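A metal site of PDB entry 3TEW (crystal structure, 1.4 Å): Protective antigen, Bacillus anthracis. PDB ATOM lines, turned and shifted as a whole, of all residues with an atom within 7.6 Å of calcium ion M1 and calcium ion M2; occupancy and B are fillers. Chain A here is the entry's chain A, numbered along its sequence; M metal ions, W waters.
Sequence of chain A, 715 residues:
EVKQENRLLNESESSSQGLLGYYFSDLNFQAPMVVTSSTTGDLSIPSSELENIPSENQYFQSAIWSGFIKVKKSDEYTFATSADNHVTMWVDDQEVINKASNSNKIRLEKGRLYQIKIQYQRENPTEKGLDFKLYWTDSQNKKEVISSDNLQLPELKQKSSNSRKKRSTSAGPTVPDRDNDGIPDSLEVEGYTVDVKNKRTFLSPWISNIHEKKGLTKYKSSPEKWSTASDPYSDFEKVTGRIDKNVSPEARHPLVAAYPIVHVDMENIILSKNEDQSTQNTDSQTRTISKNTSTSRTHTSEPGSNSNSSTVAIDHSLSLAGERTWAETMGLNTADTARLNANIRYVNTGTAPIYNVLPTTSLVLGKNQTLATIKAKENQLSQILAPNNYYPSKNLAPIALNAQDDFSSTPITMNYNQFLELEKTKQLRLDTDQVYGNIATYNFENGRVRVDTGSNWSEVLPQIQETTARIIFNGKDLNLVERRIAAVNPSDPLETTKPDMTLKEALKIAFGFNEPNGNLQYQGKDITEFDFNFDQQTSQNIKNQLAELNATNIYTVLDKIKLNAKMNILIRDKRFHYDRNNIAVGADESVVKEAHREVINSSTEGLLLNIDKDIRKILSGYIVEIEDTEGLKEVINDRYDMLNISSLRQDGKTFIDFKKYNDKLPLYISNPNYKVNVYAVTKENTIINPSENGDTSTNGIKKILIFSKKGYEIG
The backbone carbonyl oxygen (O) of Pro 223 sits close to the backbone NH (N) of Asp 179, 3.4 Å away.
The backbone NH (N) of Asp 177 lies close to the side-chain carboxylate (OD1) of Asp 185.
The backbone NH (N) of Ser 222 lies within hydrogen-bond range of the side-chain hydroxyl (OG1) of Thr 228.
OG of Ser 222 lies within hydrogen-bond range of N of Glu 224, 3.0 Å away.
The side-chain carboxylate (OD1) of Asp 235 lies within hydrogen-bond range of the backbone NH (N) of Thr 228.
The backbone carbonyl oxygen of Trp 226 sits at hydrogen-bond distance from the backbone NH of Asp 235, 2.9 Å away.
The backbone carbonyl oxygen (O) of Glu 188 is in hydrogen-bond range of the backbone NH (N) of Ser 221, 3.0 Å away.
The side-chain amino group (NZ) of Lys 225 sits at hydrogen-bond distance from the backbone carbonyl oxygen (O) of Thr 228, 2.9 Å away.
Six residues have an atom within 4 Å of calcium ion M1: Asp 179, Asp 181, Glu 188, Ser 222, Lys 225 and Asp 235.
Along chain A the residues within 4 Å of calcium ion M1 span positions 179 to 235.
Of the 26 residues printed, 5 come within 4 Å of calcium ion M2.
OD2 of Asp 181 is bound to calcium ion M1, 2.3 Å away.
Calcium ion M1 is bound by OD2 of Asp 179 (2.3 Å).
O of Ser 222 is bound to calcium ion M1 (2.3 Å).
OD2 of Asp 235 is bound to calcium ion M1 (2.4 Å).
The backbone carbonyl oxygen (O) of Lys 225 is bound to calcium ion M1, at 2.4 Å.
Calcium ion M1 is bound by OE1 of Glu 188, at 2.4 Å.
The side-chain carboxylate (OE2) of Glu 188 is bound to calcium ion M1 (2.9 Å).
O of Ile 183 binds calcium ion M2, 2.3 Å away.
OD1 of Asp 177 binds calcium ion M2 (2.3 Å).
OD1 of Asp 179 is bound to calcium ion M2, at 2.4 Å.
Calcium ion M2 is bound by OD1 of Asp 181, 2.4 Å away.
OE2 of Glu 188 is bound to calcium ion M2 (2.4 Å).
Calcium ion M2 is bound by water W1 (2.4 Å).
Water W1 lies within hydrogen-bond range of OD1 of Asp 185, O of Pro 223 and N of Arg 178.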
ATOM      1  N   TYR A  22     -25.219  31.971  10.270  1.00  0.00           N
ATOM      2  CA  TYR A  22     -25.190  31.172   9.069  1.00  0.00           C
ATOM      3  C   TYR A  22     -26.149  31.866   8.085  1.00  0.00           C
ATOM      4  O   TYR A  22     -27.309  32.074   8.427  1.00  0.00           O
ATOM      5  CB  TYR A  22     -25.688  29.766   9.364  1.00  0.00           C
ATOM      6  CG  TYR A  22     -24.824  29.026  10.364  1.00  0.00           C
ATOM      7  CD1 TYR A  22     -24.994  29.189  11.730  1.00  0.00           C
ATOM      8  CD2 TYR A  22     -23.808  28.185   9.931  1.00  0.00           C
ATOM      9  CE1 TYR A  22     -24.191  28.521  12.627  1.00  0.00           C
ATOM     10  CE2 TYR A  22     -23.011  27.515  10.815  1.00  0.00           C
ATOM     11  CZ  TYR A  22     -23.204  27.681  12.153  1.00  0.00           C
ATOM     12  OH  TYR A  22     -22.404  27.014  13.059  1.00  0.00           O
ATOM     13  N   PRO A 176     -27.178  21.438  10.083  1.00  0.00           N
ATOM     14  CA  PRO A 176     -26.537  20.144  10.309  1.00  0.00           C
ATOM     15  C   PRO A 176     -25.074  20.347  10.614  1.00  0.00           C
ATOM     16  O   PRO A 176     -24.316  20.867   9.788  1.00  0.00           O
ATOM     17  CB  PRO A 176     -26.716  19.430   8.965  1.00  0.00           C
ATOM     18  CG  PRO A 176     -27.916  20.067   8.364  1.00  0.00           C
ATOM     19  CD  PRO A 176     -27.834  21.510   8.763  1.00  0.00           C
ATOM     20  N   ASP A 177     -24.687  19.943  11.819  1.00  0.00           N
ATOM     21  CA  ASP A 177     -23.334  20.113  12.314  1.00  0.00           C
ATOM     22  C   ASP A 177     -23.097  18.955  13.291  1.00  0.00           C
ATOM     23  O   ASP A 177     -23.075  19.151  14.506  1.00  0.00           O
ATOM     24  CB  ASP A 177     -23.204  21.472  13.025  1.00  0.00           C
ATOM     25  CG  ASP A 177     -21.797  21.742  13.547  1.00  0.00           C
ATOM     26  OD1 ASP A 177     -20.861  21.098  13.054  1.00  0.00           O
ATOM     27  OD2 ASP A 177     -21.626  22.602  14.427  1.00  0.00           O
ATOM     28  N   ARG A 178     -22.931  17.770  12.710  1.00  0.00           N
ATOM     29  CA  ARG A 178     -22.876  16.515  13.469  1.00  0.00           C
ATOM     30  C   ARG A 178     -21.806  16.519  14.589  1.00  0.00           C
ATOM     31  O   ARG A 178     -21.976  15.895  15.634  1.00  0.00           O
ATOM     32  CB  ARG A 178     -22.659  15.338  12.491  1.00  0.00           C
ATOM     33  CG  ARG A 178     -23.797  15.120  11.469  1.00  0.00           C
ATOM     34  CD  ARG A 178     -23.385  14.225  10.300  1.00  0.00           C
ATOM     35  NE  ARG A 178     -23.558  12.797  10.547  1.00  0.00           N
ATOM     36  CZ  ARG A 178     -24.748  12.212  10.600  1.00  0.00           C
ATOM     37  NH1 ARG A 178     -25.829  12.945  10.452  1.00  0.00           N
ATOM     38  NH2 ARG A 178     -24.858  10.909  10.833  1.00  0.00           N
ATOM     39  N   ASP A 179     -20.692  17.196  14.372  1.00  0.00           N
ATOM     40  CA  ASP A 179     -19.594  17.153  15.358  1.00  0.00           C
ATOM     41  C   ASP A 179     -19.502  18.410  16.228  1.00  0.00           C
ATOM     42  O   ASP A 179     -18.572  18.570  17.028  1.00  0.00           O
ATOM     43  CB  ASP A 179     -18.258  16.905  14.644  1.00  0.00           C
ATOM     44  CG  ASP A 179     -17.969  17.938  13.559  1.00  0.00           C
ATOM     45  OD1 ASP A 179     -18.622  19.006  13.525  1.00  0.00           O
ATOM     46  OD2 ASP A 179     -17.083  17.679  12.740  1.00  0.00           O
ATOM     47  N   ASN A 180     -20.472  19.302  16.066  1.00  0.00           N
ATOM     48  CA  ASN A 180     -20.529  20.511  16.892  1.00  0.00           C
ATOM     49  C   ASN A 180     -19.294  21.413  16.838  1.00  0.00           C
ATOM     50  O   ASN A 180     -19.005  22.123  17.806  1.00  0.00           O
ATOM     51  CB  ASN A 180     -20.847  20.188  18.351  1.00  0.00           C
ATOM     52  CG  ASN A 180     -21.545  21.337  19.056  1.00  0.00           C
ATOM     53  OD1 ASN A 180     -22.415  21.984  18.478  1.00  0.00           O
ATOM     54  ND2 ASN A 180     -21.156  21.596  20.289  1.00  0.00           N
ATOM     55  N   ASP A 181     -18.548  21.396  15.731  1.00  0.00           N
ATOM     56  CA  ASP A 181     -17.440  22.332  15.630  1.00  0.00           C
ATOM     57  C   ASP A 181     -17.875  23.704  15.124  1.00  0.00           C
ATOM     58  O   ASP A 181     -17.124  24.658  15.274  1.00  0.00           O
ATOM     59  CB  ASP A 181     -16.225  21.773  14.860  1.00  0.00           C
ATOM     60  CG  ASP A 181     -16.535  21.366  13.404  1.00  0.00           C
ATOM     61  OD1 ASP A 181     -17.540  21.830  12.824  1.00  0.00           O
ATOM     62  OD2 ASP A 181     -15.719  20.587  12.812  1.00  0.00           O
ATOM     63  N   GLY A 182     -19.083  23.804  14.593  1.00  0.00           N
ATOM     64  CA  GLY A 182     -19.517  25.076  14.024  1.00  0.00           C
ATOM     65  C   GLY A 182     -19.567  25.107  12.509  1.00  0.00           C
ATOM     66  O   GLY A 182     -20.337  25.884  11.928  1.00  0.00           O
ATOM     67  N   ILE A 183     -18.799  24.270  11.823  1.00  0.00           N
ATOM     68  CA  ILE A 183     -18.820  24.272  10.363  1.00  0.00           C
ATOM     69  C   ILE A 183     -19.874  23.277   9.884  1.00  0.00           C
ATOM     70  O   ILE A 183     -19.849  22.108  10.272  1.00  0.00           O
ATOM     71  CB  ILE A 183     -17.463  23.829   9.764  1.00  0.00           C
ATOM     72  CG1 ILE A 183     -16.290  24.611  10.382  1.00  0.00           C
ATOM     73  CG2 ILE A 183     -17.499  24.004   8.247  1.00  0.00           C
ATOM     74  CD1 ILE A 183     -14.946  24.043   9.973  1.00  0.00           C
ATOM     75  N   PRO A 184     -20.834  23.740   9.065  1.00  0.00           N
ATOM     76  CA  PRO A 184     -21.896  22.848   8.603  1.00  0.00           C
ATOM     77  C   PRO A 184     -21.359  21.606   7.909  1.00  0.00           C
ATOM     78  O   PRO A 184     -20.332  21.714   7.231  1.00  0.00           O
ATOM     79  CB  PRO A 184     -22.646  23.717   7.594  1.00  0.00           C
ATOM     80  CG  PRO A 184     -22.499  25.114   8.137  1.00  0.00           C
ATOM     81  CD  PRO A 184     -21.064  25.139   8.634  1.00  0.00           C
ATOM     82  N   ASP A 185     -22.041  20.471   8.079  1.00  0.00           N
ATOM     83  CA  ASP A 185     -21.623  19.186   7.509  1.00  0.00           C
ATOM     84  C   ASP A 185     -21.250  19.369   6.032  1.00  0.00           C
ATOM     85  O   ASP A 185     -20.195  18.915   5.588  1.00  0.00           O
ATOM     86  CB  ASP A 185     -22.762  18.143   7.516  1.00  0.00           C
ATOM     87  CG  ASP A 185     -23.271  17.744   8.910  1.00  0.00           C
ATOM     88  OD1 ASP A 185     -22.662  18.065   9.955  1.00  0.00           O
ATOM     89  OD2 ASP A 185     -24.320  17.058   8.958  1.00  0.00           O
ATOM     90  N   SER A 186     -22.140  19.997   5.259  1.00  0.00           N
ATOM     91  CA  SER A 186     -21.979  20.097   3.816  1.00  0.00           C
ATOM     92  C   SER A 186     -20.724  20.857   3.393  1.00  0.00           C
ATOM     93  O   SER A 186     -20.077  20.503   2.398  1.00  0.00           O
ATOM     94  CB  SER A 186     -23.227  20.691   3.151  1.00  0.00           C
ATOM     95  OG  SER A 186     -23.464  22.028   3.563  1.00  0.00           O
ATOM     96  N   GLU A 188     -17.930  21.101   5.144  1.00  0.00           N
ATOM     97  CA  GLU A 188     -16.744  20.313   5.482  1.00  0.00           C
ATOM     98  C   GLU A 188     -16.483  19.260   4.420  1.00  0.00           C
ATOM     99  O   GLU A 188     -15.341  18.996   4.057  1.00  0.00           O
ATOM    100  CB  GLU A 188     -16.919  19.651   6.827  1.00  0.00           C
ATOM    101  CG  GLU A 188     -16.917  20.644   7.953  1.00  0.00           C
ATOM    102  CD  GLU A 188     -16.556  19.981   9.274  1.00  0.00           C
ATOM    103  OE1 GLU A 188     -15.367  19.690   9.471  1.00  0.00           O
ATOM    104  OE2 GLU A 188     -17.433  19.725  10.104  1.00  0.00           O
ATOM    105  N   TYR A 192     -14.374  24.319   1.627  1.00  0.00           N
ATOM    106  CA  TYR A 192     -14.649  25.671   2.088  1.00  0.00           C
ATOM    107  C   TYR A 192     -13.390  26.516   2.112  1.00  0.00           C
ATOM    108  O   TYR A 192     -12.269  26.014   2.077  1.00  0.00           O
ATOM    109  CB  TYR A 192     -15.293  25.686   3.473  1.00  0.00           C
ATOM    110  CG  TYR A 192     -14.536  24.952   4.574  1.00  0.00           C
ATOM    111  CD1 TYR A 192     -14.606  23.564   4.681  1.00  0.00           C
ATOM    112  CD2 TYR A 192     -13.796  25.645   5.525  1.00  0.00           C
ATOM    113  CE1 TYR A 192     -13.979  22.899   5.699  1.00  0.00           C
ATOM    114  CE2 TYR A 192     -13.143  24.976   6.563  1.00  0.00           C
ATOM    115  CZ  TYR A 192     -13.243  23.598   6.626  1.00  0.00           C
ATOM    116  OH  TYR A 192     -12.603  22.934   7.638  1.00  0.00           O
ATOM    117  N   SER A 221     -12.722  18.849   5.583  1.00  0.00           N
ATOM    118  CA  SER A 221     -12.515  18.254   6.898  1.00  0.00           C
ATOM    119  C   SER A 221     -13.641  17.246   7.150  1.00  0.00           C
ATOM    120  O   SER A 221     -14.562  17.126   6.337  1.00  0.00           O
ATOM    121  CB  SER A 221     -12.411  19.347   7.962  1.00  0.00           C
ATOM    122  OG  SER A 221     -13.442  20.333   7.853  1.00  0.00           O
ATOM    123  N   SER A 222     -13.513  16.434   8.199  1.00  0.00           N
ATOM    124  CA  SER A 222     -14.593  15.485   8.480  1.00  0.00           C
ATOM    125  C   SER A 222     -15.742  16.169   9.227  1.00  0.00           C
ATOM    126  O   SER A 222     -15.518  16.831  10.253  1.00  0.00           O
ATOM    127  CB  SER A 222     -14.098  14.332   9.342  1.00  0.00           C
ATOM    128  OG  SER A 222     -15.239  13.591   9.769  1.00  0.00           O
ATOM    129  N   PRO A 223     -16.977  15.987   8.730  1.00  0.00           N
ATOM    130  CA  PRO A 223     -18.150  16.527   9.411  1.00  0.00           C
ATOM    131  C   PRO A 223     -18.507  15.738  10.678  1.00  0.00           C
ATOM    132  O   PRO A 223     -19.435  16.119  11.385  1.00  0.00           O
ATOM    133  CB  PRO A 223     -19.266  16.349   8.371  1.00  0.00           C
ATOM    134  CG  PRO A 223     -18.850  15.110   7.625  1.00  0.00           C
ATOM    135  CD  PRO A 223     -17.340  15.217   7.522  1.00  0.00           C
ATOM    136  N   GLU A 224     -17.780  14.660  10.950  1.00  0.00           N
ATOM    137  CA  GLU A 224     -18.027  13.825  12.122  1.00  0.00           C
ATOM    138  C   GLU A 224     -16.885  13.832  13.148  1.00  0.00           C
ATOM    139  O   GLU A 224     -16.966  13.175  14.195  1.00  0.00           O
ATOM    140  CB  GLU A 224     -18.345  12.410  11.693  1.00  0.00           C
ATOM    141  CG  GLU A 224     -19.711  12.399  10.974  1.00  0.00           C
ATOM    142  CD  GLU A 224     -20.230  11.040  10.620  1.00  0.00           C
ATOM    143  OE1 GLU A 224     -19.751  10.047  11.203  1.00  0.00           O
ATOM    144  OE2 GLU A 224     -21.143  10.975   9.762  1.00  0.00           O
ATOM    145  N   LYS A 225     -15.841  14.584  12.857  1.00  0.00           N
ATOM    146  CA  LYS A 225     -14.755  14.798  13.809  1.00  0.00           C
ATOM    147  C   LYS A 225     -14.626  16.276  14.146  1.00  0.00           C
ATOM    148  O   LYS A 225     -14.334  17.091  13.236  1.00  0.00           O
ATOM    149  CB  LYS A 225     -13.426  14.280  13.262  1.00  0.00           C
ATOM    150  CG  LYS A 225     -13.456  12.794  12.885  1.00  0.00           C
ATOM    151  CD  LYS A 225     -12.101  12.304  12.376  1.00  0.00           C
ATOM    152  CE  LYS A 225     -11.105  12.249  13.552  1.00  0.00           C
ATOM    153  NZ  LYS A 225      -9.746  11.899  13.175  1.00  0.00           N
ATOM    154  N   TRP A 226     -14.772  16.597  15.407  1.00  0.00           N
ATOM    155  CA  TRP A 226     -14.652  17.967  15.913  1.00  0.00           C
ATOM    156  C   TRP A 226     -13.262  18.503  15.550  1.00  0.00           C
ATOM    157  O   TRP A 226     -13.129  19.642  15.079  1.00  0.00           O
ATOM    158  CB  TRP A 226     -14.914  17.947  17.408  1.00  0.00           C
ATOM    159  CG  TRP A 226     -14.810  19.235  18.130  1.00  0.00           C
ATOM    160  CD1 TRP A 226     -15.804  20.190  18.281  1.00  0.00           C
ATOM    161  CD2 TRP A 226     -13.687  19.700  18.832  1.00  0.00           C
ATOM    162  NE1 TRP A 226     -15.315  21.222  19.056  1.00  0.00           N
ATOM    163  CE2 TRP A 226     -14.014  20.950  19.394  1.00  0.00           C
ATOM    164  CE3 TRP A 226     -12.397  19.185  19.035  1.00  0.00           C
ATOM    165  CZ2 TRP A 226     -13.102  21.700  20.151  1.00  0.00           C
ATOM    166  CZ3 TRP A 226     -11.486  19.935  19.793  1.00  0.00           C
ATOM    167  CH2 TRP A 226     -11.847  21.179  20.333  1.00  0.00           C
ATOM    168  N   SER A 227     -12.239  17.668  15.723  1.00  0.00           N
ATOM    169  CA  SER A 227     -10.881  17.946  15.199  1.00  0.00           C
ATOM    170  C   SER A 227     -10.545  16.834  14.253  1.00  0.00           C
ATOM    171  O   SER A 227     -10.410  15.681  14.687  1.00  0.00           O
ATOM    172  CB  SER A 227      -9.828  17.999  16.318  1.00  0.00           C
ATOM    173  OG  SER A 227      -8.524  18.073  15.747  1.00  0.00           O
ATOM    174  N   THR A 228     -10.453  17.154  12.974  1.00  0.00           N
ATOM    175  CA  THR A 228     -10.214  16.108  11.977  1.00  0.00           C
ATOM    176  C   THR A 228      -8.860  15.426  12.179  1.00  0.00           C
ATOM    177  O   THR A 228      -8.730  14.243  11.841  1.00  0.00           O
ATOM    178  CB  THR A 228     -10.434  16.657  10.557  1.00  0.00           C
ATOM    179  OG1 THR A 228     -11.819  16.982  10.428  1.00  0.00           O
ATOM    180  CG2 THR A 228     -10.103  15.590   9.508  1.00  0.00           C
ATOM    181  N   SER A 234     -10.417  22.535  17.396  1.00  0.00           N
ATOM    182  CA  SER A 234     -11.448  22.142  16.440  1.00  0.00           C
ATOM    183  C   SER A 234     -11.164  22.664  15.042  1.00  0.00           C
ATOM    184  O   SER A 234     -10.365  23.598  14.818  1.00  0.00           O
ATOM    185  CB  SER A 234     -12.827  22.642  16.888  1.00  0.00           C
ATOM    186  OG  SER A 234     -13.112  23.901  16.285  1.00  0.00           O
ATOM    187  N   ASP A 235     -11.824  22.036  14.079  1.00  0.00           N
ATOM    188  CA  ASP A 235     -11.652  22.447  12.678  1.00  0.00           C
ATOM    189  C   ASP A 235     -11.999  23.926  12.517  1.00  0.00           C
ATOM    190  O   ASP A 235     -11.319  24.676  11.776  1.00  0.00           O
ATOM    191  CB  ASP A 235     -12.513  21.560  11.784  1.00  0.00           C
ATOM    192  CG  ASP A 235     -12.080  20.098  11.802  1.00  0.00           C
ATOM    193  OD1 ASP A 235     -10.906  19.783  12.124  1.00  0.00           O
ATOM    194  OD2 ASP A 235     -12.961  19.266  11.446  1.00  0.00           O
ATOM    195  N   PHE A 236     -13.049  24.348  13.221  1.00  0.00           N
ATOM    196  CA  PHE A 236     -13.508  25.749  13.212  1.00  0.00           C
ATOM    197  C   PHE A 236     -12.559  26.700  13.937  1.00  0.00           C
ATOM    198  O   PHE A 236     -12.236  27.787  13.419  1.00  0.00           O
ATOM    199  CB  PHE A 236     -14.919  25.791  13.808  1.00  0.00           C
ATOM    200  CG  PHE A 236     -15.538  27.165  13.845  1.00  0.00           C
ATOM    201  CD1 PHE A 236     -16.103  27.717  12.712  1.00  0.00           C
ATOM    202  CD2 PHE A 236     -15.595  27.869  15.037  1.00  0.00           C
ATOM    203  CE1 PHE A 236     -16.719  28.970  12.753  1.00  0.00           C
ATOM    204  CE2 PHE A 236     -16.217  29.125  15.097  1.00  0.00           C
ATOM    205  CZ  PHE A 236     -16.782  29.672  13.933  1.00  0.00           C
ATOM    206  N   PRO A 254      -7.138  22.124   9.087  1.00  0.00           N
ATOM    207  CA  PRO A 254      -7.794  21.032   9.823  1.00  0.00           C
ATOM    208  C   PRO A 254      -7.198  19.668   9.523  1.00  0.00           C
ATOM    209  O   PRO A 254      -7.464  18.739  10.328  1.00  0.00           O
ATOM    210  CB  PRO A 254      -9.250  21.105   9.319  1.00  0.00           C
ATOM    211  CG  PRO A 254      -9.439  22.564   9.001  1.00  0.00           C
ATOM    212  CD  PRO A 254      -8.114  22.965   8.367  1.00  0.00           C
HETATM  213 CA    CA M   1     -15.246  18.670  11.688  1.00  0.00          CA
HETATM  214 CA    CA M   2     -19.074  20.429  11.692  1.00  0.00          CA
HETATM  215  O   HOH W   1     -20.277  18.495  10.827  1.00  0.00           O
